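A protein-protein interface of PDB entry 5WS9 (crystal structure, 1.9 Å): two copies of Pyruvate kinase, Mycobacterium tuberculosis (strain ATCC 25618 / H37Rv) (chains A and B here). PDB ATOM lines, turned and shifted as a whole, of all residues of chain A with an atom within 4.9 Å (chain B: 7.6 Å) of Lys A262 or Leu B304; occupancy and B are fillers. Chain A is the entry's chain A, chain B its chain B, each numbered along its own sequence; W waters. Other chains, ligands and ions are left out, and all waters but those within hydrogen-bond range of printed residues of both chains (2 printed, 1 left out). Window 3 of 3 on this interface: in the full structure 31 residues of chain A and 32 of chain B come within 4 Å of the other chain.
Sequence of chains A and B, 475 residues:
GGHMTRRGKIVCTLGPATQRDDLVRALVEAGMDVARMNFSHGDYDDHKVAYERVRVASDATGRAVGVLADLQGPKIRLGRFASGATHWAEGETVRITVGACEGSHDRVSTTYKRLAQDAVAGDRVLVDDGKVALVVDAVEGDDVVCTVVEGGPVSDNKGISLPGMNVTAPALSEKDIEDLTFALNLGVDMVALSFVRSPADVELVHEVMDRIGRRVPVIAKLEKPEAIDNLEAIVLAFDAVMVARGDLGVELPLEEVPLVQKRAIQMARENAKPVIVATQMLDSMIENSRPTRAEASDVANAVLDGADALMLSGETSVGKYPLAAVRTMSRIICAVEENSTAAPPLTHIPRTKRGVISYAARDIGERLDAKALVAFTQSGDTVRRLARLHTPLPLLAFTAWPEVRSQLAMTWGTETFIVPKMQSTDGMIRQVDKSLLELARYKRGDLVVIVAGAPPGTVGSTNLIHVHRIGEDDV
Of the 10 printed residues of chain A, 4 touch a printed residue of chain B.
Printed residues of chain A that touch a printed residue of chain B: Pro A258, Leu A259, Lys A262 and Arg A263.
Hydrophobic or aromatic side chains of chain A within 4 Å of the printed part of chain B: Pro A258 and Leu A259.
Hydrophobic or aromatic side chains of chain B within 4 Å of the printed part of chain A: Ala B300 and Leu B304.
Among the printed residues, no Asp or Glu carboxylate lies within 4 Å of a Lys or Arg side-chain nitrogen of the other chain.
Of chain B, only Asn B301 (2.9 Å) and Leu B304 (3.6 Å) come within 4 Å of Lys A262.
Leu B304 touches just one residue of chain A: Lys A262.
Printed residues of chain A within 4 Å of Asn B301: Lys A262.
Of the printed residues of chain A, Ser B297 touches Pro A258.
Printed residues of chain B within 4 Å of Leu A259: Asn B339.
Of the printed residues of chain B, Pro A258 touches Ser B297 and Ala B300.
Glu B337 touches none of the printed residues of chain A.
Ala B302 touches none of the printed residues of chain A.
The nearest residue of chain B that does not touch Lys A262 is Ala B300 (5.8 Å).
The nearest printed residue of chain B that does not touch Arg A263 is Val B336 (7.2 Å).
Pro A258 touches Ser B297 (CG to CA, 3.99 Å).
Ala B300 touches Pro A258 (CB to CB, 3.4 Å).
CB of Asn B339 touches CD1 of Leu A259, 3.4 Å away.
Lys A262 touches Leu B304.
Positions printed for both chains: 262, 265 and 305.
Of the 6 pairs that touch across the chains among the printed residues, none has its exchanged pair printed and touching as well.
NH2 of Arg A263 sits close to ND2 of Asn B339, at 3.2 Å.
The side-chain amide oxygen (OD1) of Asn B301 sits at hydrogen-bond distance from the side-chain amino group (NZ) of Lys A262 (2.9 Å).
The backbone carbonyl oxygen of Ser B297 is in hydrogen-bond range of the side-chain amide nitrogen of Asn B301 (2.9 Å).
NZ of Lys A262 is in salt-bridge range of OD1 of Asp A305 (2.7 Å).
Water W1 bridges the side-chain amide nitrogen of Gln A261 (2.9 Å) and the side-chain hydroxyl of Ser B297 (3.2 Å).
Water W2 lies within hydrogen-bond range of OD1 of Asp A305 (2.9 Å), NZ of Lys A262 (3.2 Å) and OD1 of Asn B301 (3.4 Å).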
ATOM      1  N   PRO A 258      11.203  -6.897 -15.226  1.00  0.00           N
ATOM      2  CA  PRO A 258      11.375  -8.169 -15.975  1.00  0.00           C
ATOM      3  C   PRO A 258      12.778  -8.389 -16.530  1.00  0.00           C
ATOM      4  O   PRO A 258      13.361  -9.472 -16.330  1.00  0.00           O
ATOM      5  CB  PRO A 258      10.313  -8.076 -17.073  1.00  0.00           C
ATOM      6  CG  PRO A 258       9.233  -7.271 -16.433  1.00  0.00           C
ATOM      7  CD  PRO A 258       9.969  -6.193 -15.647  1.00  0.00           C
ATOM      8  N   LEU A 259      13.401  -7.364 -17.061  1.00  0.00           N
ATOM      9  CA  LEU A 259      14.746  -7.563 -17.549  1.00  0.00           C
ATOM     10  C   LEU A 259      15.788  -7.615 -16.406  1.00  0.00           C
ATOM     11  O   LEU A 259      16.774  -8.328 -16.482  1.00  0.00           O
ATOM     12  CB  LEU A 259      15.085  -6.531 -18.598  1.00  0.00           C
ATOM     13  CG  LEU A 259      14.400  -6.749 -19.951  1.00  0.00           C
ATOM     14  CD1 LEU A 259      14.926  -5.693 -20.935  1.00  0.00           C
ATOM     15  CD2 LEU A 259      14.685  -8.140 -20.497  1.00  0.00           C
ATOM     16  N   VAL A 260      15.534  -6.910 -15.307  1.00  0.00           N
ATOM     17  CA  VAL A 260      16.405  -7.050 -14.151  1.00  0.00           C
ATOM     18  C   VAL A 260      16.396  -8.475 -13.645  1.00  0.00           C
ATOM     19  O   VAL A 260      17.474  -9.052 -13.420  1.00  0.00           O
ATOM     20  CB  VAL A 260      16.057  -6.044 -13.036  1.00  0.00           C
ATOM     21  CG1 VAL A 260      16.764  -6.398 -11.762  1.00  0.00           C
ATOM     22  CG2 VAL A 260      16.489  -4.640 -13.472  1.00  0.00           C
ATOM     23  N   GLN A 261      15.198  -9.059 -13.499  1.00  0.00           N
ATOM     24  CA  GLN A 261      15.031 -10.427 -13.055  1.00  0.00           C
ATOM     25  C   GLN A 261      15.894 -11.363 -13.885  1.00  0.00           C
ATOM     26  O   GLN A 261      16.654 -12.197 -13.350  1.00  0.00           O
ATOM     27  CB  GLN A 261      13.555 -10.851 -13.131  1.00  0.00           C
ATOM     28  CG  GLN A 261      13.351 -12.344 -12.921  1.00  0.00           C
ATOM     29  CD  GLN A 261      11.901 -12.781 -12.931  1.00  0.00           C
ATOM     30  OE1 GLN A 261      11.042 -12.141 -12.293  1.00  0.00           O
ATOM     31  NE2 GLN A 261      11.618 -13.910 -13.611  1.00  0.00           N
ATOM     32  N   LYS A 262      15.799 -11.216 -15.193  1.00  0.00           N
ATOM     33  CA  LYS A 262      16.512 -12.103 -16.102  1.00  0.00           C
ATOM     34  C   LYS A 262      18.024 -11.931 -16.020  1.00  0.00           C
ATOM     35  O   LYS A 262      18.782 -12.948 -15.988  1.00  0.00           O
ATOM     36  CB  LYS A 262      16.015 -11.921 -17.529  1.00  0.00           C
ATOM     37  CG  LYS A 262      14.568 -12.414 -17.696  1.00  0.00           C
ATOM     38  CD  LYS A 262      13.960 -11.920 -18.994  1.00  0.00           C
ATOM     39  CE  LYS A 262      12.505 -12.285 -19.116  1.00  0.00           C
ATOM     40  NZ  LYS A 262      12.421 -13.684 -19.575  1.00  0.00           N
ATOM     41  N   ARG A 263      18.469 -10.685 -15.896  1.00  0.00           N
ATOM     42  CA  ARG A 263      19.897 -10.414 -15.689  1.00  0.00           C
ATOM     43  C   ARG A 263      20.432 -11.031 -14.381  1.00  0.00           C
ATOM     44  O   ARG A 263      21.539 -11.532 -14.328  1.00  0.00           O
ATOM     45  CB  ARG A 263      20.181  -8.911 -15.709  1.00  0.00           C
ATOM     46  CG  ARG A 263      19.895  -8.276 -17.056  1.00  0.00           C
ATOM     47  CD  ARG A 263      20.410  -6.862 -17.160  1.00  0.00           C
ATOM     48  NE  ARG A 263      19.898  -6.256 -18.377  1.00  0.00           N
ATOM     49  CZ  ARG A 263      18.926  -5.339 -18.428  1.00  0.00           C
ATOM     50  NH1 ARG A 263      18.343  -4.894 -17.311  1.00  0.00           N
ATOM     51  NH2 ARG A 263      18.534  -4.860 -19.604  1.00  0.00           N
ATOM     52  N   ALA A 264      19.640 -10.942 -13.332  1.00  0.00           N
ATOM     53  CA  ALA A 264      20.067 -11.413 -12.021  1.00  0.00           C
ATOM     54  C   ALA A 264      20.162 -12.932 -11.985  1.00  0.00           C
ATOM     55  O   ALA A 264      21.090 -13.490 -11.414  1.00  0.00           O
ATOM     56  CB  ALA A 264      19.129 -10.901 -10.941  1.00  0.00           C
ATOM     57  N   ILE A 265      19.206 -13.596 -12.603  1.00  0.00           N
ATOM     58  CA  ILE A 265      19.232 -15.045 -12.712  1.00  0.00           C
ATOM     59  C   ILE A 265      20.469 -15.513 -13.486  1.00  0.00           C
ATOM     60  O   ILE A 265      21.175 -16.419 -13.050  1.00  0.00           O
ATOM     61  CB  ILE A 265      17.928 -15.584 -13.363  1.00  0.00           C
ATOM     62  CG1 ILE A 265      16.745 -15.374 -12.403  1.00  0.00           C
ATOM     63  CG2 ILE A 265      18.048 -17.073 -13.648  1.00  0.00           C
ATOM     64  CD1 ILE A 265      15.402 -15.574 -13.074  1.00  0.00           C
ATOM     65  N   GLN A 266      20.742 -14.877 -14.611  1.00  0.00           N
ATOM     66  CA  GLN A 266      21.888 -15.226 -15.421  1.00  0.00           C
ATOM     67  C   GLN A 266      23.182 -15.039 -14.640  1.00  0.00           C
ATOM     68  O   GLN A 266      24.042 -15.918 -14.639  1.00  0.00           O
ATOM     69  CB  GLN A 266      21.933 -14.379 -16.671  1.00  0.00           C
ATOM     70  CG  GLN A 266      23.035 -14.758 -17.650  1.00  0.00           C
ATOM     71  CD  GLN A 266      22.709 -16.025 -18.461  1.00  0.00           C
ATOM     72  OE1 GLN A 266      21.539 -16.391 -18.629  1.00  0.00           O
ATOM     73  NE2 GLN A 266      23.748 -16.689 -18.972  1.00  0.00           N
ATOM     74  N   ASP A 305      13.755 -18.961 -17.518  1.00  0.00           N
ATOM     75  CA  ASP A 305      14.830 -17.980 -17.305  1.00  0.00           C
ATOM     76  C   ASP A 305      16.041 -18.673 -16.653  1.00  0.00           C
ATOM     77  O   ASP A 305      17.128 -18.142 -16.679  1.00  0.00           O
ATOM     78  CB  ASP A 305      14.391 -16.891 -16.302  1.00  0.00           C
ATOM     79  CG  ASP A 305      13.420 -15.848 -16.879  1.00  0.00           C
ATOM     80  OD1 ASP A 305      13.328 -15.707 -18.117  1.00  0.00           O
ATOM     81  OD2 ASP A 305      12.778 -15.122 -16.046  1.00  0.00           O
ATOM     82  N   LYS B 262       3.695 -19.870 -26.521  1.00  0.00           N
ATOM     83  CA  LYS B 262       4.991 -19.709 -27.200  1.00  0.00           C
ATOM     84  C   LYS B 262       5.037 -20.461 -28.538  1.00  0.00           C
ATOM     85  O   LYS B 262       5.510 -19.899 -29.554  1.00  0.00           O
ATOM     86  CB  LYS B 262       6.134 -20.142 -26.284  1.00  0.00           C
ATOM     87  CG  LYS B 262       6.305 -19.183 -25.104  1.00  0.00           C
ATOM     88  CD  LYS B 262       7.173 -19.769 -24.011  1.00  0.00           C
ATOM     89  CE  LYS B 262       7.219 -18.897 -22.771  1.00  0.00           C
ATOM     90  NZ  LYS B 262       8.183 -17.813 -22.996  1.00  0.00           N
ATOM     91  N   ILE B 265       2.786 -18.423 -31.102  1.00  0.00           N
ATOM     92  CA  ILE B 265       3.490 -17.236 -31.573  1.00  0.00           C
ATOM     93  C   ILE B 265       4.540 -17.599 -32.623  1.00  0.00           C
ATOM     94  O   ILE B 265       4.616 -16.967 -33.686  1.00  0.00           O
ATOM     95  CB  ILE B 265       4.118 -16.444 -30.398  1.00  0.00           C
ATOM     96  CG1 ILE B 265       3.007 -15.812 -29.532  1.00  0.00           C
ATOM     97  CG2 ILE B 265       4.987 -15.314 -30.925  1.00  0.00           C
ATOM     98  CD1 ILE B 265       3.511 -15.319 -28.200  1.00  0.00           C
ATOM     99  N   ARG B 269       4.568 -16.485 -36.654  1.00  0.00           N
ATOM    100  CA  ARG B 269       5.709 -15.801 -37.237  1.00  0.00           C
ATOM    101  C   ARG B 269       6.346 -16.566 -38.406  1.00  0.00           C
ATOM    102  O   ARG B 269       6.706 -15.951 -39.419  1.00  0.00           O
ATOM    103  CB  ARG B 269       6.771 -15.508 -36.182  1.00  0.00           C
ATOM    104  CG  ARG B 269       6.416 -14.330 -35.311  1.00  0.00           C
ATOM    105  CD  ARG B 269       7.492 -14.113 -34.248  1.00  0.00           C
ATOM    106  NE  ARG B 269       8.771 -13.769 -34.857  1.00  0.00           N
ATOM    107  CZ  ARG B 269       9.919 -14.416 -34.694  1.00  0.00           C
ATOM    108  NH1 ARG B 269      10.017 -15.482 -33.914  1.00  0.00           N
ATOM    109  NH2 ARG B 269      10.999 -13.981 -35.325  1.00  0.00           N
ATOM    110  N   SER B 297       5.616  -9.042 -15.772  1.00  0.00           N
ATOM    111  CA  SER B 297       6.423 -10.103 -16.331  1.00  0.00           C
ATOM    112  C   SER B 297       5.740 -10.745 -17.583  1.00  0.00           C
ATOM    113  O   SER B 297       6.386 -11.064 -18.610  1.00  0.00           O
ATOM    114  CB  SER B 297       6.643 -11.160 -15.260  1.00  0.00           C
ATOM    115  OG  SER B 297       7.184 -12.351 -15.786  1.00  0.00           O
ATOM    116  N   ASP B 298       4.459 -11.005 -17.454  1.00  0.00           N
ATOM    117  CA  ASP B 298       3.667 -11.603 -18.511  1.00  0.00           C
ATOM    118  C   ASP B 298       3.686 -10.733 -19.775  1.00  0.00           C
ATOM    119  O   ASP B 298       3.950 -11.228 -20.862  1.00  0.00           O
ATOM    120  CB  ASP B 298       2.254 -11.818 -18.015  1.00  0.00           C
ATOM    121  CG  ASP B 298       1.365 -12.473 -19.022  1.00  0.00           C
ATOM    122  OD1 ASP B 298       1.757 -13.479 -19.623  1.00  0.00           O
ATOM    123  OD2 ASP B 298       0.233 -11.983 -19.200  1.00  0.00           O
ATOM    124  N   VAL B 299       3.526  -9.429 -19.604  1.00  0.00           N
ATOM    125  CA  VAL B 299       3.594  -8.491 -20.747  1.00  0.00           C
ATOM    126  C   VAL B 299       4.993  -8.496 -21.378  1.00  0.00           C
ATOM    127  O   VAL B 299       5.133  -8.682 -22.580  1.00  0.00           O
ATOM    128  CB  VAL B 299       3.191  -7.083 -20.327  1.00  0.00           C
ATOM    129  CG1 VAL B 299       3.475  -6.083 -21.412  1.00  0.00           C
ATOM    130  CG2 VAL B 299       1.733  -7.053 -19.918  1.00  0.00           C
ATOM    131  N   ALA B 300       6.019  -8.363 -20.559  1.00  0.00           N
ATOM    132  CA  ALA B 300       7.414  -8.403 -21.069  1.00  0.00           C
ATOM    133  C   ALA B 300       7.712  -9.681 -21.808  1.00  0.00           C
ATOM    134  O   ALA B 300       8.341  -9.653 -22.880  1.00  0.00           O
ATOM    135  CB  ALA B 300       8.402  -8.214 -19.935  1.00  0.00           C
ATOM    136  N   ASN B 301       7.269 -10.810 -21.264  1.00  0.00           N
ATOM    137  CA  ASN B 301       7.599 -12.103 -21.861  1.00  0.00           C
ATOM    138  C   ASN B 301       6.845 -12.362 -23.168  1.00  0.00           C
ATOM    139  O   ASN B 301       7.397 -13.015 -24.084  1.00  0.00           O
ATOM    140  CB  ASN B 301       7.393 -13.246 -20.848  1.00  0.00           C
ATOM    141  CG  ASN B 301       8.595 -13.412 -19.942  1.00  0.00           C
ATOM    142  OD1 ASN B 301       9.675 -13.761 -20.428  1.00  0.00           O
ATOM    143  ND2 ASN B 301       8.432 -13.150 -18.613  1.00  0.00           N
ATOM    144  N   ALA B 302       5.621 -11.845 -23.272  1.00  0.00           N
ATOM    145  CA  ALA B 302       4.888 -11.912 -24.541  1.00  0.00           C
ATOM    146  C   ALA B 302       5.582 -11.100 -25.625  1.00  0.00           C
ATOM    147  O   ALA B 302       5.660 -11.540 -26.797  1.00  0.00           O
ATOM    148  CB  ALA B 302       3.414 -11.488 -24.339  1.00  0.00           C
ATOM    149  N   VAL B 303       6.209  -9.988 -25.239  1.00  0.00           N
ATOM    150  CA  VAL B 303       7.067  -9.233 -26.170  1.00  0.00           C
ATOM    151  C   VAL B 303       8.280 -10.056 -26.629  1.00  0.00           C
ATOM    152  O   VAL B 303       8.552 -10.167 -27.821  1.00  0.00           O
ATOM    153  CB  VAL B 303       7.556  -7.899 -25.553  1.00  0.00           C
ATOM    154  CG1 VAL B 303       8.553  -7.185 -26.480  1.00  0.00           C
ATOM    155  CG2 VAL B 303       6.377  -6.983 -25.263  1.00  0.00           C
ATOM    156  N   LEU B 304       8.983 -10.639 -25.667  1.00  0.00           N
ATOM    157  CA  LEU B 304      10.172 -11.448 -25.953  1.00  0.00           C
ATOM    158  C   LEU B 304       9.851 -12.678 -26.752  1.00  0.00           C
ATOM    159  O   LEU B 304      10.686 -13.141 -27.539  1.00  0.00           O
ATOM    160  CB  LEU B 304      10.872 -11.850 -24.642  1.00  0.00           C
ATOM    161  CG  LEU B 304      11.450 -10.663 -23.881  1.00  0.00           C
ATOM    162  CD1 LEU B 304      11.790 -11.060 -22.446  1.00  0.00           C
ATOM    163  CD2 LEU B 304      12.672 -10.120 -24.598  1.00  0.00           C
ATOM    164  N   ASP B 305       8.657 -13.218 -26.557  1.00  0.00           N
ATOM    165  CA  ASP B 305       8.203 -14.425 -27.266  1.00  0.00           C
ATOM    166  C   ASP B 305       8.076 -14.128 -28.772  1.00  0.00           C
ATOM    167  O   ASP B 305       8.037 -15.039 -29.565  1.00  0.00           O
ATOM    168  CB  ASP B 305       6.798 -14.833 -26.791  1.00  0.00           C
ATOM    169  CG  ASP B 305       6.770 -15.525 -25.419  1.00  0.00           C
ATOM    170  OD1 ASP B 305       7.836 -16.019 -24.939  1.00  0.00           O
ATOM    171  OD2 ASP B 305       5.640 -15.610 -24.839  1.00  0.00           O
ATOM    172  N   GLY B 306       7.846 -12.855 -29.117  1.00  0.00           N
ATOM    173  CA  GLY B 306       7.680 -12.453 -30.512  1.00  0.00           C
ATOM    174  C   GLY B 306       6.245 -12.083 -30.940  1.00  0.00           C
ATOM    175  O   GLY B 306       5.968 -12.009 -32.136  1.00  0.00           O
ATOM    176  N   ALA B 307       5.370 -11.755 -29.998  1.00  0.00           N
ATOM    177  CA  ALA B 307       3.987 -11.400 -30.324  1.00  0.00           C
ATOM    178  C   ALA B 307       3.923 -10.084 -31.099  1.00  0.00           C
ATOM    179  O   ALA B 307       4.688  -9.109 -30.781  1.00  0.00           O
ATOM    180  CB  ALA B 307       3.139 -11.283 -29.060  1.00  0.00           C
ATOM    181  N   VAL B 336      11.176  -3.219 -22.733  1.00  0.00           N
ATOM    182  CA  VAL B 336      11.784  -4.432 -23.283  1.00  0.00           C
ATOM    183  C   VAL B 336      12.436  -4.137 -24.603  1.00  0.00           C
ATOM    184  O   VAL B 336      13.555  -4.519 -24.840  1.00  0.00           O
ATOM    185  CB  VAL B 336      10.757  -5.559 -23.460  1.00  0.00           C
ATOM    186  CG1 VAL B 336      11.395  -6.750 -24.175  1.00  0.00           C
ATOM    187  CG2 VAL B 336      10.212  -5.966 -22.106  1.00  0.00           C
ATOM    188  N   GLU B 337      11.698  -3.433 -25.483  1.00  0.00           N
ATOM    189  CA  GLU B 337      12.187  -3.112 -26.814  1.00  0.00           C
ATOM    190  C   GLU B 337      13.422  -2.240 -26.808  1.00  0.00           C
ATOM    191  O   GLU B 337      14.272  -2.371 -27.686  1.00  0.00           O
ATOM    192  CB  GLU B 337      11.084  -2.464 -27.631  1.00  0.00           C
ATOM    193  CG  GLU B 337      10.000  -3.440 -28.056  1.00  0.00           C
ATOM    194  CD  GLU B 337       8.773  -2.767 -28.655  1.00  0.00           C
ATOM    195  OE1 GLU B 337       8.750  -1.526 -28.783  1.00  0.00           O
ATOM    196  OE2 GLU B 337       7.855  -3.503 -29.027  1.00  0.00           O
ATOM    197  N   ASN B 339      15.858  -2.362 -24.744  1.00  0.00           N
ATOM    198  CA  ASN B 339      16.949  -3.304 -24.590  1.00  0.00           C
ATOM    199  C   ASN B 339      17.274  -4.038 -25.899  1.00  0.00           C
ATOM    200  O   ASN B 339      18.405  -4.067 -26.328  1.00  0.00           O
ATOM    201  CB  ASN B 339      16.613  -4.326 -23.498  1.00  0.00           C
ATOM    202  CG  ASN B 339      17.697  -5.393 -23.339  1.00  0.00           C
ATOM    203  OD1 ASN B 339      17.522  -6.560 -23.728  1.00  0.00           O
ATOM    204  ND2 ASN B 339      18.795  -5.006 -22.793  1.00  0.00           N
ATOM    205  N   SER B 340      16.258  -4.643 -26.511  1.00  0.00           N
ATOM    206  CA  SER B 340      16.427  -5.326 -27.792  1.00  0.00           C
ATOM    207  C   SER B 340      15.088  -5.662 -28.403  1.00  0.00           C
ATOM    208  O   SER B 340      14.120  -5.941 -27.675  1.00  0.00           O
ATOM    209  CB  SER B 340      17.229  -6.604 -27.568  1.00  0.00           C
ATOM    210  OG  SER B 340      17.130  -7.486 -28.646  1.00  0.00           O
ATOM    211  N   THR B 341      15.007  -5.612 -29.737  1.00  0.00           N
ATOM    212  CA  THR B 341      13.811  -6.049 -30.448  1.00  0.00           C
ATOM    213  C   THR B 341      13.884  -7.528 -30.884  1.00  0.00           C
ATOM    214  O   THR B 341      12.970  -8.017 -31.565  1.00  0.00           O
ATOM    215  CB  THR B 341      13.533  -5.204 -31.730  1.00  0.00           C
ATOM    216  OG1 THR B 341      14.667  -5.222 -32.592  1.00  0.00           O
ATOM    217  CG2 THR B 341      13.209  -3.752 -31.369  1.00  0.00           C
ATOM    218  N   ALA B 342      14.979  -8.221 -30.544  1.00  0.00           N
ATOM    219  CA  ALA B 342      15.190  -9.582 -31.044  1.00  0.00           C
ATOM    220  C   ALA B 342      14.026 -10.503 -30.667  1.00  0.00           C
ATOM    221  O   ALA B 342      13.491 -10.442 -29.547  1.00  0.00           O
ATOM    222  CB  ALA B 342      16.515 -10.153 -30.525  1.00  0.00           C
ATOM    223  N   ALA B 343      13.613 -11.319 -31.626  1.00  0.00           N
ATOM    224  CA  ALA B 343      12.651 -12.393 -31.394  1.00  0.00           C
ATOM    225  C   ALA B 343      13.375 -13.744 -31.537  1.00  0.00           C
ATOM    226  O   ALA B 343      14.484 -13.792 -32.010  1.00  0.00           O
ATOM    227  CB  ALA B 343      11.541 -12.291 -32.411  1.00  0.00           C
ATOM    228  N   PRO B 344      12.720 -14.837 -31.156  1.00  0.00           N
ATOM    229  CA  PRO B 344      13.349 -16.144 -31.404  1.00  0.00           C
ATOM    230  C   PRO B 344      13.584 -16.363 -32.899  1.00  0.00           C
ATOM    231  O   PRO B 344      12.780 -15.955 -33.724  1.00  0.00           O
ATOM    232  CB  PRO B 344      12.324 -17.144 -30.845  1.00  0.00           C
ATOM    233  CG  PRO B 344      11.506 -16.344 -29.855  1.00  0.00           C
ATOM    234  CD  PRO B 344      11.453 -14.945 -30.405  1.00  0.00           C
ATOM    235  N   HIS B 390      11.504  -8.906 -37.006  1.00  0.00           N
ATOM    236  CA  HIS B 390      11.890  -7.899 -36.046  1.00  0.00           C
ATOM    237  C   HIS B 390      13.181  -7.216 -36.560  1.00  0.00           C
ATOM    238  O   HIS B 390      14.021  -7.835 -37.210  1.00  0.00           O
ATOM    239  CB  HIS B 390      12.031  -8.475 -34.631  1.00  0.00           C
ATOM    240  CG  HIS B 390      10.709  -8.805 -33.961  1.00  0.00           C
ATOM    241  ND1 HIS B 390      10.487  -8.634 -32.610  1.00  0.00           N
ATOM    242  CD2 HIS B 390       9.533  -9.248 -34.477  1.00  0.00           C
ATOM    243  CE1 HIS B 390       9.244  -8.985 -32.320  1.00  0.00           C
ATOM    244  NE2 HIS B 390       8.638  -9.334 -33.441  1.00  0.00           N
HETATM  245  O   HOH W   1       8.965 -14.595 -14.419  1.00  0.00           O
HETATM  246  O   HOH W   2      11.420 -16.641 -20.031  1.00  0.00           O
